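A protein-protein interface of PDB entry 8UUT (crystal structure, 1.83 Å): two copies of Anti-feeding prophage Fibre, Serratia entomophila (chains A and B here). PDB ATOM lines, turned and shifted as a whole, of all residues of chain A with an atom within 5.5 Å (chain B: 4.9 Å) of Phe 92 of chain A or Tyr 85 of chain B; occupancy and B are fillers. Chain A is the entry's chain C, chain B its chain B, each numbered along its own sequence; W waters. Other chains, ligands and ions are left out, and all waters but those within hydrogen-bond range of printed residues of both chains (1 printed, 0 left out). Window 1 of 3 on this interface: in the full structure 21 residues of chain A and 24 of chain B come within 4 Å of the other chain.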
ATOM      1  N   TYR A  70     -23.223 -18.234  24.907  1.00  0.00           N
ATOM      2  CA  TYR A  70     -22.272 -18.471  25.981  1.00  0.00           C
ATOM      3  C   TYR A  70     -22.123 -19.929  26.389  1.00  0.00           C
ATOM      4  O   TYR A  70     -21.266 -20.226  27.231  1.00  0.00           O
ATOM      5  CB  TYR A  70     -22.680 -17.640  27.210  1.00  0.00           C
ATOM      6  CG  TYR A  70     -22.727 -16.177  26.858  1.00  0.00           C
ATOM      7  CD1 TYR A  70     -21.559 -15.498  26.535  1.00  0.00           C
ATOM      8  CD2 TYR A  70     -23.939 -15.504  26.751  1.00  0.00           C
ATOM      9  CE1 TYR A  70     -21.587 -14.166  26.181  1.00  0.00           C
ATOM     10  CE2 TYR A  70     -23.980 -14.181  26.389  1.00  0.00           C
ATOM     11  CZ  TYR A  70     -22.799 -13.518  26.103  1.00  0.00           C
ATOM     12  OH  TYR A  70     -22.822 -12.193  25.746  1.00  0.00           O
ATOM     13  N   GLY A  88     -18.534 -24.682  26.694  1.00  0.00           N
ATOM     14  CA  GLY A  88     -18.618 -23.242  26.819  1.00  0.00           C
ATOM     15  C   GLY A  88     -18.517 -22.556  25.473  1.00  0.00           C
ATOM     16  O   GLY A  88     -18.001 -23.118  24.508  1.00  0.00           O
ATOM     17  N   ARG A  89     -19.020 -21.320  25.416  1.00  0.00           N
ATOM     18  CA  ARG A  89     -18.970 -20.505  24.205  1.00  0.00           C
ATOM     19  C   ARG A  89     -18.703 -19.060  24.595  1.00  0.00           C
ATOM     20  O   ARG A  89     -19.043 -18.625  25.698  1.00  0.00           O
ATOM     21  CB  ARG A  89     -20.287 -20.548  23.388  1.00  0.00           C
ATOM     22  CG  ARG A  89     -20.869 -21.932  23.086  1.00  0.00           C
ATOM     23  CD  ARG A  89     -22.082 -21.811  22.162  1.00  0.00           C
ATOM     24  NE  ARG A  89     -21.689 -21.595  20.768  1.00  0.00           N
ATOM     25  CZ  ARG A  89     -22.218 -20.695  19.944  1.00  0.00           C
ATOM     26  NH1 ARG A  89     -23.159 -19.853  20.362  1.00  0.00           N
ATOM     27  NH2 ARG A  89     -21.790 -20.631  18.685  1.00  0.00           N
ATOM     28  N   GLY A  90     -18.108 -18.314  23.670  1.00  0.00           N
ATOM     29  CA  GLY A  90     -17.999 -16.872  23.850  1.00  0.00           C
ATOM     30  C   GLY A  90     -17.286 -16.444  25.114  1.00  0.00           C
ATOM     31  O   GLY A  90     -17.686 -15.450  25.739  1.00  0.00           O
ATOM     32  N   ALA A  91     -16.242 -17.179  25.508  1.00  0.00           N
ATOM     33  CA  ALA A  91     -15.410 -16.946  26.688  1.00  0.00           C
ATOM     34  C   ALA A  91     -16.109 -17.311  27.988  1.00  0.00           C
ATOM     35  O   ALA A  91     -15.548 -17.077  29.079  1.00  0.00           O
ATOM     36  CB  ALA A  91     -14.902 -15.498  26.768  1.00  0.00           C
ATOM     37  N   PHE A  92     -17.294 -17.907  27.918  1.00  0.00           N
ATOM     38  CA  PHE A  92     -18.044 -18.273  29.105  1.00  0.00           C
ATOM     39  C   PHE A  92     -18.130 -19.788  29.242  1.00  0.00           C
ATOM     40  O   PHE A  92     -17.726 -20.542  28.356  1.00  0.00           O
ATOM     41  CB  PHE A  92     -19.440 -17.635  29.078  1.00  0.00           C
ATOM     42  CG  PHE A  92     -19.447 -16.223  29.593  1.00  0.00           C
ATOM     43  CD1 PHE A  92     -18.896 -15.195  28.835  1.00  0.00           C
ATOM     44  CD2 PHE A  92     -19.957 -15.928  30.856  1.00  0.00           C
ATOM     45  CE1 PHE A  92     -18.874 -13.893  29.315  1.00  0.00           C
ATOM     46  CE2 PHE A  92     -19.931 -14.626  31.346  1.00  0.00           C
ATOM     47  CZ  PHE A  92     -19.390 -13.607  30.573  1.00  0.00           C
ATOM     48  N   TYR A  93     -18.626 -20.213  30.404  1.00  0.00           N
ATOM     49  CA  TYR A  93     -18.821 -21.616  30.750  1.00  0.00           C
ATOM     50  C   TYR A  93     -19.929 -21.668  31.798  1.00  0.00           C
ATOM     51  O   TYR A  93     -20.355 -20.631  32.313  1.00  0.00           O
ATOM     52  CB  TYR A  93     -17.516 -22.253  31.253  1.00  0.00           C
ATOM     53  CG  TYR A  93     -16.999 -21.688  32.569  1.00  0.00           C
ATOM     54  CD1 TYR A  93     -17.479 -22.154  33.792  1.00  0.00           C
ATOM     55  CD2 TYR A  93     -16.020 -20.699  32.586  1.00  0.00           C
ATOM     56  CE1 TYR A  93     -17.012 -21.647  34.981  1.00  0.00           C
ATOM     57  CE2 TYR A  93     -15.543 -20.189  33.781  1.00  0.00           C
ATOM     58  CZ  TYR A  93     -16.043 -20.663  34.968  1.00  0.00           C
ATOM     59  OH  TYR A  93     -15.580 -20.157  36.156  1.00  0.00           O
ATOM     60  N   LEU A  94     -20.413 -22.875  32.108  1.00  0.00           N
ATOM     61  CA  LEU A  94     -21.472 -23.039  33.099  1.00  0.00           C
ATOM     62  C   LEU A  94     -20.895 -23.346  34.477  1.00  0.00           C
ATOM     63  O   LEU A  94     -20.058 -24.243  34.627  1.00  0.00           O
ATOM     64  CB  LEU A  94     -22.467 -24.138  32.696  1.00  0.00           C
ATOM     65  CG  LEU A  94     -23.263 -23.942  31.401  1.00  0.00           C
ATOM     66  CD1 LEU A  94     -24.434 -24.917  31.378  1.00  0.00           C
ATOM     67  CD2 LEU A  94     -23.768 -22.500  31.256  1.00  0.00           C
ATOM     68  N   ARG A 142     -23.806 -18.501  34.135  1.00  0.00           N
ATOM     69  CA  ARG A 142     -22.647 -18.543  33.260  1.00  0.00           C
ATOM     70  C   ARG A 142     -21.525 -17.716  33.873  1.00  0.00           C
ATOM     71  O   ARG A 142     -21.765 -16.647  34.440  1.00  0.00           O
ATOM     72  CB  ARG A 142     -23.003 -18.053  31.848  1.00  0.00           C
ATOM     73  CG  ARG A 142     -23.583 -16.649  31.749  1.00  0.00           C
ATOM     74  CD  ARG A 142     -23.798 -16.293  30.302  1.00  0.00           C
ATOM     75  NE  ARG A 142     -24.563 -15.064  30.097  1.00  0.00           N
ATOM     76  CZ  ARG A 142     -24.019 -13.891  29.797  1.00  0.00           C
ATOM     77  NH1 ARG A 142     -22.710 -13.781  29.671  1.00  0.00           N
ATOM     78  NH2 ARG A 142     -24.786 -12.825  29.615  1.00  0.00           N
ATOM     79  N   LYS A 143     -20.303 -18.227  33.777  1.00  0.00           N
ATOM     80  CA  LYS A 143     -19.141 -17.556  34.329  1.00  0.00           C
ATOM     81  C   LYS A 143     -18.078 -17.458  33.248  1.00  0.00           C
ATOM     82  O   LYS A 143     -18.170 -18.092  32.198  1.00  0.00           O
ATOM     83  CB  LYS A 143     -18.611 -18.291  35.566  1.00  0.00           C
ATOM     84  CG  LYS A 143     -19.521 -18.142  36.777  1.00  0.00           C
ATOM     85  CD  LYS A 143     -19.098 -19.042  37.918  1.00  0.00           C
ATOM     86  CE  LYS A 143     -20.092 -18.926  39.084  1.00  0.00           C
ATOM     87  NZ  LYS A 143     -19.780 -19.895  40.179  1.00  0.00           N
ATOM     88  N   SER A 144     -17.078 -16.623  33.490  1.00  0.00           N
ATOM     89  CA  SER A 144     -15.970 -16.477  32.560  1.00  0.00           C
ATOM     90  C   SER A 144     -14.678 -16.457  33.354  1.00  0.00           C
ATOM     91  O   SER A 144     -14.600 -15.816  34.404  1.00  0.00           O
ATOM     92  CB  SER A 144     -16.069 -15.198  31.719  1.00  0.00           C
ATOM     93  OG  SER A 144     -14.927 -15.093  30.877  1.00  0.00           O
ATOM     94  N   SER A 149     -17.271 -12.451  37.229  1.00  0.00           N
ATOM     95  CA  SER A 149     -18.683 -12.244  36.968  1.00  0.00           C
ATOM     96  C   SER A 149     -19.447 -13.566  37.030  1.00  0.00           C
ATOM     97  O   SER A 149     -18.879 -14.655  36.915  1.00  0.00           O
ATOM     98  CB  SER A 149     -18.877 -11.575  35.607  1.00  0.00           C
ATOM     99  OG  SER A 149     -18.539 -12.463  34.556  1.00  0.00           O
ATOM    100  N   ILE A 151     -23.554 -14.606  35.680  1.00  0.00           N
ATOM    101  CA  ILE A 151     -24.742 -14.050  35.048  1.00  0.00           C
ATOM    102  C   ILE A 151     -25.794 -15.142  34.900  1.00  0.00           C
ATOM    103  O   ILE A 151     -25.482 -16.256  34.457  1.00  0.00           O
ATOM    104  CB  ILE A 151     -24.393 -13.411  33.687  1.00  0.00           C
ATOM    105  CG1 ILE A 151     -23.320 -12.344  33.902  1.00  0.00           C
ATOM    106  CG2 ILE A 151     -25.616 -12.806  33.027  1.00  0.00           C
ATOM    107  CD1 ILE A 151     -22.715 -11.816  32.628  1.00  0.00           C
ATOM    108  N   HIS B  60     -17.609 -22.988  19.637  1.00  0.00           N
ATOM    109  CA  HIS B  60     -17.232 -22.137  20.755  1.00  0.00           C
ATOM    110  C   HIS B  60     -17.479 -20.670  20.469  1.00  0.00           C
ATOM    111  O   HIS B  60     -17.158 -19.833  21.313  1.00  0.00           O
ATOM    112  CB  HIS B  60     -15.756 -22.353  21.115  1.00  0.00           C
ATOM    113  CG  HIS B  60     -15.464 -23.715  21.666  1.00  0.00           C
ATOM    114  ND1 HIS B  60     -15.928 -24.134  22.893  1.00  0.00           N
ATOM    115  CD2 HIS B  60     -14.743 -24.747  21.166  1.00  0.00           C
ATOM    116  CE1 HIS B  60     -15.514 -25.365  23.125  1.00  0.00           C
ATOM    117  NE2 HIS B  60     -14.793 -25.762  22.093  1.00  0.00           N
ATOM    118  N   CYS B  72      -4.850 -27.683  19.298  1.00  0.00           N
ATOM    119  CA  CYS B  72      -5.522 -26.538  18.716  1.00  0.00           C
ATOM    120  C   CYS B  72      -6.221 -25.770  19.828  1.00  0.00           C
ATOM    121  O   CYS B  72      -6.511 -26.309  20.901  1.00  0.00           O
ATOM    122  CB  CYS B  72      -6.502 -26.950  17.612  1.00  0.00           C
ATOM    123  SG  CYS B  72      -7.756 -28.126  18.110  1.00  0.00           S
ATOM    124  N   ALA B  73      -6.474 -24.495  19.574  1.00  0.00           N
ATOM    125  CA  ALA B  73      -7.097 -23.652  20.588  1.00  0.00           C
ATOM    126  C   ALA B  73      -7.976 -22.620  19.895  1.00  0.00           C
ATOM    127  O   ALA B  73      -7.547 -21.987  18.925  1.00  0.00           O
ATOM    128  CB  ALA B  73      -6.029 -22.974  21.467  1.00  0.00           C
ATOM    129  N   PHE B  74      -9.196 -22.452  20.400  1.00  0.00           N
ATOM    130  CA  PHE B  74     -10.208 -21.585  19.806  1.00  0.00           C
ATOM    131  C   PHE B  74     -10.514 -20.457  20.782  1.00  0.00           C
ATOM    132  O   PHE B  74     -10.949 -20.715  21.910  1.00  0.00           O
ATOM    133  CB  PHE B  74     -11.446 -22.417  19.460  1.00  0.00           C
ATOM    134  CG  PHE B  74     -11.106 -23.589  18.599  1.00  0.00           C
ATOM    135  CD1 PHE B  74     -10.918 -23.421  17.237  1.00  0.00           C
ATOM    136  CD2 PHE B  74     -10.868 -24.833  19.157  1.00  0.00           C
ATOM    137  CE1 PHE B  74     -10.541 -24.496  16.437  1.00  0.00           C
ATOM    138  CE2 PHE B  74     -10.487 -25.902  18.361  1.00  0.00           C
ATOM    139  CZ  PHE B  74     -10.324 -25.725  16.999  1.00  0.00           C
ATOM    140  N   CYS B  76     -12.019 -16.731  22.202  1.00  0.00           N
ATOM    141  CA  CYS B  76     -13.070 -15.720  22.237  1.00  0.00           C
ATOM    142  C   CYS B  76     -12.618 -14.517  23.053  1.00  0.00           C
ATOM    143  O   CYS B  76     -12.015 -14.673  24.117  1.00  0.00           O
ATOM    144  CB  CYS B  76     -14.356 -16.257  22.856  1.00  0.00           C
ATOM    145  SG  CYS B  76     -14.919 -17.818  22.186  1.00  0.00           S
ATOM    146  N   TYR B  78     -13.648 -11.108  25.280  1.00  0.00           N
ATOM    147  CA  TYR B  78     -14.741 -10.654  26.128  1.00  0.00           C
ATOM    148  C   TYR B  78     -14.184  -9.702  27.166  1.00  0.00           C
ATOM    149  O   TYR B  78     -13.095  -9.931  27.699  1.00  0.00           O
ATOM    150  CB  TYR B  78     -15.457 -11.813  26.835  1.00  0.00           C
ATOM    151  CG  TYR B  78     -16.393 -11.365  27.946  1.00  0.00           C
ATOM    152  CD1 TYR B  78     -17.624 -10.798  27.653  1.00  0.00           C
ATOM    153  CD2 TYR B  78     -16.047 -11.518  29.281  1.00  0.00           C
ATOM    154  CE1 TYR B  78     -18.492 -10.387  28.664  1.00  0.00           C
ATOM    155  CE2 TYR B  78     -16.910 -11.116  30.303  1.00  0.00           C
ATOM    156  CZ  TYR B  78     -18.127 -10.549  29.983  1.00  0.00           C
ATOM    157  OH  TYR B  78     -18.990 -10.151  30.990  1.00  0.00           O
ATOM    158  N   VAL B  83     -10.439 -15.964  26.162  1.00  0.00           N
ATOM    159  CA  VAL B  83     -10.485 -17.340  26.644  1.00  0.00           C
ATOM    160  C   VAL B  83     -10.228 -18.237  25.453  1.00  0.00           C
ATOM    161  O   VAL B  83     -10.729 -17.963  24.359  1.00  0.00           O
ATOM    162  CB  VAL B  83     -11.849 -17.688  27.277  1.00  0.00           C
ATOM    163  CG1 VAL B  83     -11.981 -19.202  27.477  1.00  0.00           C
ATOM    164  CG2 VAL B  83     -12.050 -16.925  28.584  1.00  0.00           C
ATOM    165  N   ALA B  84      -9.434 -19.294  25.651  1.00  0.00           N
ATOM    166  CA  ALA B  84      -9.238 -20.306  24.622  1.00  0.00           C
ATOM    167  C   ALA B  84      -9.780 -21.649  25.102  1.00  0.00           C
ATOM    168  O   ALA B  84      -9.544 -22.056  26.242  1.00  0.00           O
ATOM    169  CB  ALA B  84      -7.757 -20.448  24.245  1.00  0.00           C
ATOM    170  N   TYR B  85     -10.511 -22.332  24.226  1.00  0.00           N
ATOM    171  CA  TYR B  85     -10.946 -23.698  24.460  1.00  0.00           C
ATOM    172  C   TYR B  85      -9.991 -24.607  23.702  1.00  0.00           C
ATOM    173  O   TYR B  85      -9.779 -24.420  22.497  1.00  0.00           O
ATOM    174  CB  TYR B  85     -12.393 -23.892  23.996  1.00  0.00           C
ATOM    175  CG  TYR B  85     -13.354 -22.889  24.599  1.00  0.00           C
ATOM    176  CD1 TYR B  85     -14.038 -23.170  25.780  1.00  0.00           C
ATOM    177  CD2 TYR B  85     -13.567 -21.650  23.994  1.00  0.00           C
ATOM    178  CE1 TYR B  85     -14.929 -22.256  26.335  1.00  0.00           C
ATOM    179  CE2 TYR B  85     -14.455 -20.731  24.539  1.00  0.00           C
ATOM    180  CZ  TYR B  85     -15.126 -21.032  25.705  1.00  0.00           C
ATOM    181  OH  TYR B  85     -15.993 -20.103  26.228  1.00  0.00           O
ATOM    182  N   VAL B  86      -9.405 -25.577  24.412  1.00  0.00           N
ATOM    183  CA  VAL B  86      -8.179 -26.250  23.984  1.00  0.00           C
ATOM    184  C   VAL B  86      -8.412 -27.738  23.789  1.00  0.00           C
ATOM    185  O   VAL B  86      -9.068 -28.391  24.614  1.00  0.00           O
ATOM    186  CB  VAL B  86      -7.044 -26.029  25.009  1.00  0.00           C
ATOM    187  CG1 VAL B  86      -5.752 -26.688  24.520  1.00  0.00           C
ATOM    188  CG2 VAL B  86      -6.849 -24.533  25.247  1.00  0.00           C
ATOM    189  N   TYR B  87      -7.832 -28.276  22.709  1.00  0.00           N
ATOM    190  CA  TYR B  87      -7.875 -29.691  22.368  1.00  0.00           C
ATOM    191  C   TYR B  87      -6.483 -30.182  22.009  1.00  0.00           C
ATOM    192  O   TYR B  87      -5.712 -29.468  21.359  1.00  0.00           O
ATOM    193  CB  TYR B  87      -8.821 -29.944  21.187  1.00  0.00           C
ATOM    194  CG  TYR B  87     -10.233 -29.492  21.501  1.00  0.00           C
ATOM    195  CD1 TYR B  87     -10.616 -28.162  21.331  1.00  0.00           C
ATOM    196  CD2 TYR B  87     -11.168 -30.388  21.983  1.00  0.00           C
ATOM    197  CE1 TYR B  87     -11.896 -27.736  21.635  1.00  0.00           C
ATOM    198  CE2 TYR B  87     -12.459 -29.971  22.281  1.00  0.00           C
ATOM    199  CZ  TYR B  87     -12.804 -28.648  22.112  1.00  0.00           C
ATOM    200  OH  TYR B  87     -14.080 -28.231  22.404  1.00  0.00           O
ATOM    201  N   THR B 123      -7.707 -27.753  29.099  1.00  0.00           N
ATOM    202  CA  THR B 123      -8.946 -27.758  28.338  1.00  0.00           C
ATOM    203  C   THR B 123      -9.538 -26.371  28.152  1.00  0.00           C
ATOM    204  O   THR B 123     -10.318 -26.171  27.214  1.00  0.00           O
ATOM    205  CB  THR B 123      -9.984 -28.688  28.994  1.00  0.00           C
ATOM    206  OG1 THR B 123     -10.169 -28.340  30.377  1.00  0.00           O
ATOM    207  CG2 THR B 123      -9.502 -30.101  28.918  1.00  0.00           C
ATOM    208  N   MET B 124      -9.169 -25.406  28.993  1.00  0.00           N
ATOM    209  CA  MET B 124      -9.614 -24.030  28.849  1.00  0.00           C
ATOM    210  C   MET B 124      -8.611 -23.153  29.574  1.00  0.00           C
ATOM    211  O   MET B 124      -8.029 -23.577  30.577  1.00  0.00           O
ATOM    212  CB  MET B 124     -11.045 -23.842  29.369  1.00  0.00           C
ATOM    213  CG  MET B 124     -11.654 -22.471  29.069  1.00  0.00           C
ATOM    214  SD  MET B 124     -13.207 -22.156  29.955  1.00  0.00           S
ATOM    215  CE  MET B 124     -14.123 -23.642  29.626  1.00  0.00           C
HETATM  216  O   HOH W   1     -14.146 -18.833  30.520  1.00  0.00           O
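SG of Cys 76 of chain B sits close to N of Ala 91 of chain A (3.6 Å).
N of Gly 90 of chain A is in hydrogen-bond range of SG of Cys 76 of chain B.
The backbone carbonyl oxygen (O) of Gly 88 of chain A lies within hydrogen-bond range of a ring nitrogen (ND1) of His 60 of chain B (2.8 Å).
The backbone carbonyl oxygen (O) of Phe 92 of chain A sits at hydrogen-bond distance from the side-chain hydroxyl (OH) of Tyr 85 of chain B, 2.8 Å away.
The side-chain hydroxyl (OH) of Tyr 85 of chain B lies close to the backbone NH (N) of Arg 89 of chain A (3.4 Å).
The backbone NH (N) of Gly 90 of chain A sits at hydrogen-bond distance from the backbone carbonyl oxygen (O) of His 60 of chain B, 3.0 Å away.
The backbone NH (N) of Ala 91 of chain A sits at hydrogen-bond distance from the side-chain hydroxyl (OH) of Tyr 85 of chain B, at 3.0 Å.
OG of Ser 144 of chain A is in hydrogen-bond range of O of Ala 91 of chain A, at 2.7 Å.
NE2 of His 60 of chain B lies within hydrogen-bond range of OH of Tyr 87 of chain B (2.6 Å).
The side-chain sulfur of Cys 76 of chain B is in hydrogen-bond range of the backbone carbonyl oxygen of His 60 of chain B (3.1 Å).
The backbone carbonyl oxygen (O) of Phe 74 of chain B lies within hydrogen-bond range of the backbone NH (N) of Tyr 85 of chain B (2.9 Å).
The backbone carbonyl oxygen (O) of Tyr 70 of chain A lies within hydrogen-bond range of the backbone NH (N) of Arg 89 of chain A.
The backbone NH (N) of Cys 76 of chain B sits at hydrogen-bond distance from the backbone carbonyl oxygen (O) of Val 83 of chain B (2.8 Å).
Tyr 85 of chain B touches Gly 88 of chain A (OH to C, 3.6 Å).
CA of Arg 89 of chain A touches O of His 60 of chain B, at 3.5 Å.
Gly 90 of chain A touches Tyr 85 of chain B.
Ala 91 of chain A touches Tyr 78 of chain B.
Val 83 of chain B touches Ala 91 of chain A.
Phe 92 of chain A touches Tyr 78 of chain B (CZ to CZ, 3.4 Å).
Printed residues of chain B within 4 Å of Ala 91 of chain A: Cys 76, Tyr 78, Val 83 and Tyr 85.
Of the printed residues of chain B, Phe 92 of chain A touches Tyr 78 and Tyr 85.
Printed residues of chain A within 4 Å of Val 83 of chain B: Ala 91 (3.5 Å).
Ala 84 of chain B touches none of the printed residues of chain A.
Tyr 85 of chain B touches just these residues of chain A: Gly 88 (3.6 Å), Arg 89 (3.3 Å), Gly 90 (3.8 Å), Ala 91 (3.0 Å) and Phe 92 (2.8 Å).
The nearest residue of chain A that does not touch Tyr 85 of chain B is Tyr 93 of chain A (4.9 Å).
The nearest printed residue of chain A that does not touch Cys 76 of chain B is Arg 89 of chain A (4.7 Å).
Of the 13 printed residues of chain B, 5 touch a printed residue of chain A.
Hydrophobic or aromatic side chains of chain B that line the printed part of chain A: His 60, Tyr 78, Val 83 and Tyr 85.
Of the 13 printed residues of chain A, 5 touch a printed residue of chain B.
Printed residues of chain A that touch a printed residue of chain B: Gly 88, Arg 89, Gly 90, Ala 91 and Phe 92.
Along chain A the printed residues that touch a printed residue of chain B span positions 88 to 92.
Among the printed residues, no Asp or Glu carboxylate lies within 4 Å of a Lys or Arg side-chain nitrogen of the other chain.
No position is printed for both chains.
Water W1 bridges O of Ala 91 of chain A (2.7 Å) and SD of Met 124 of chain B (3.5 Å).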
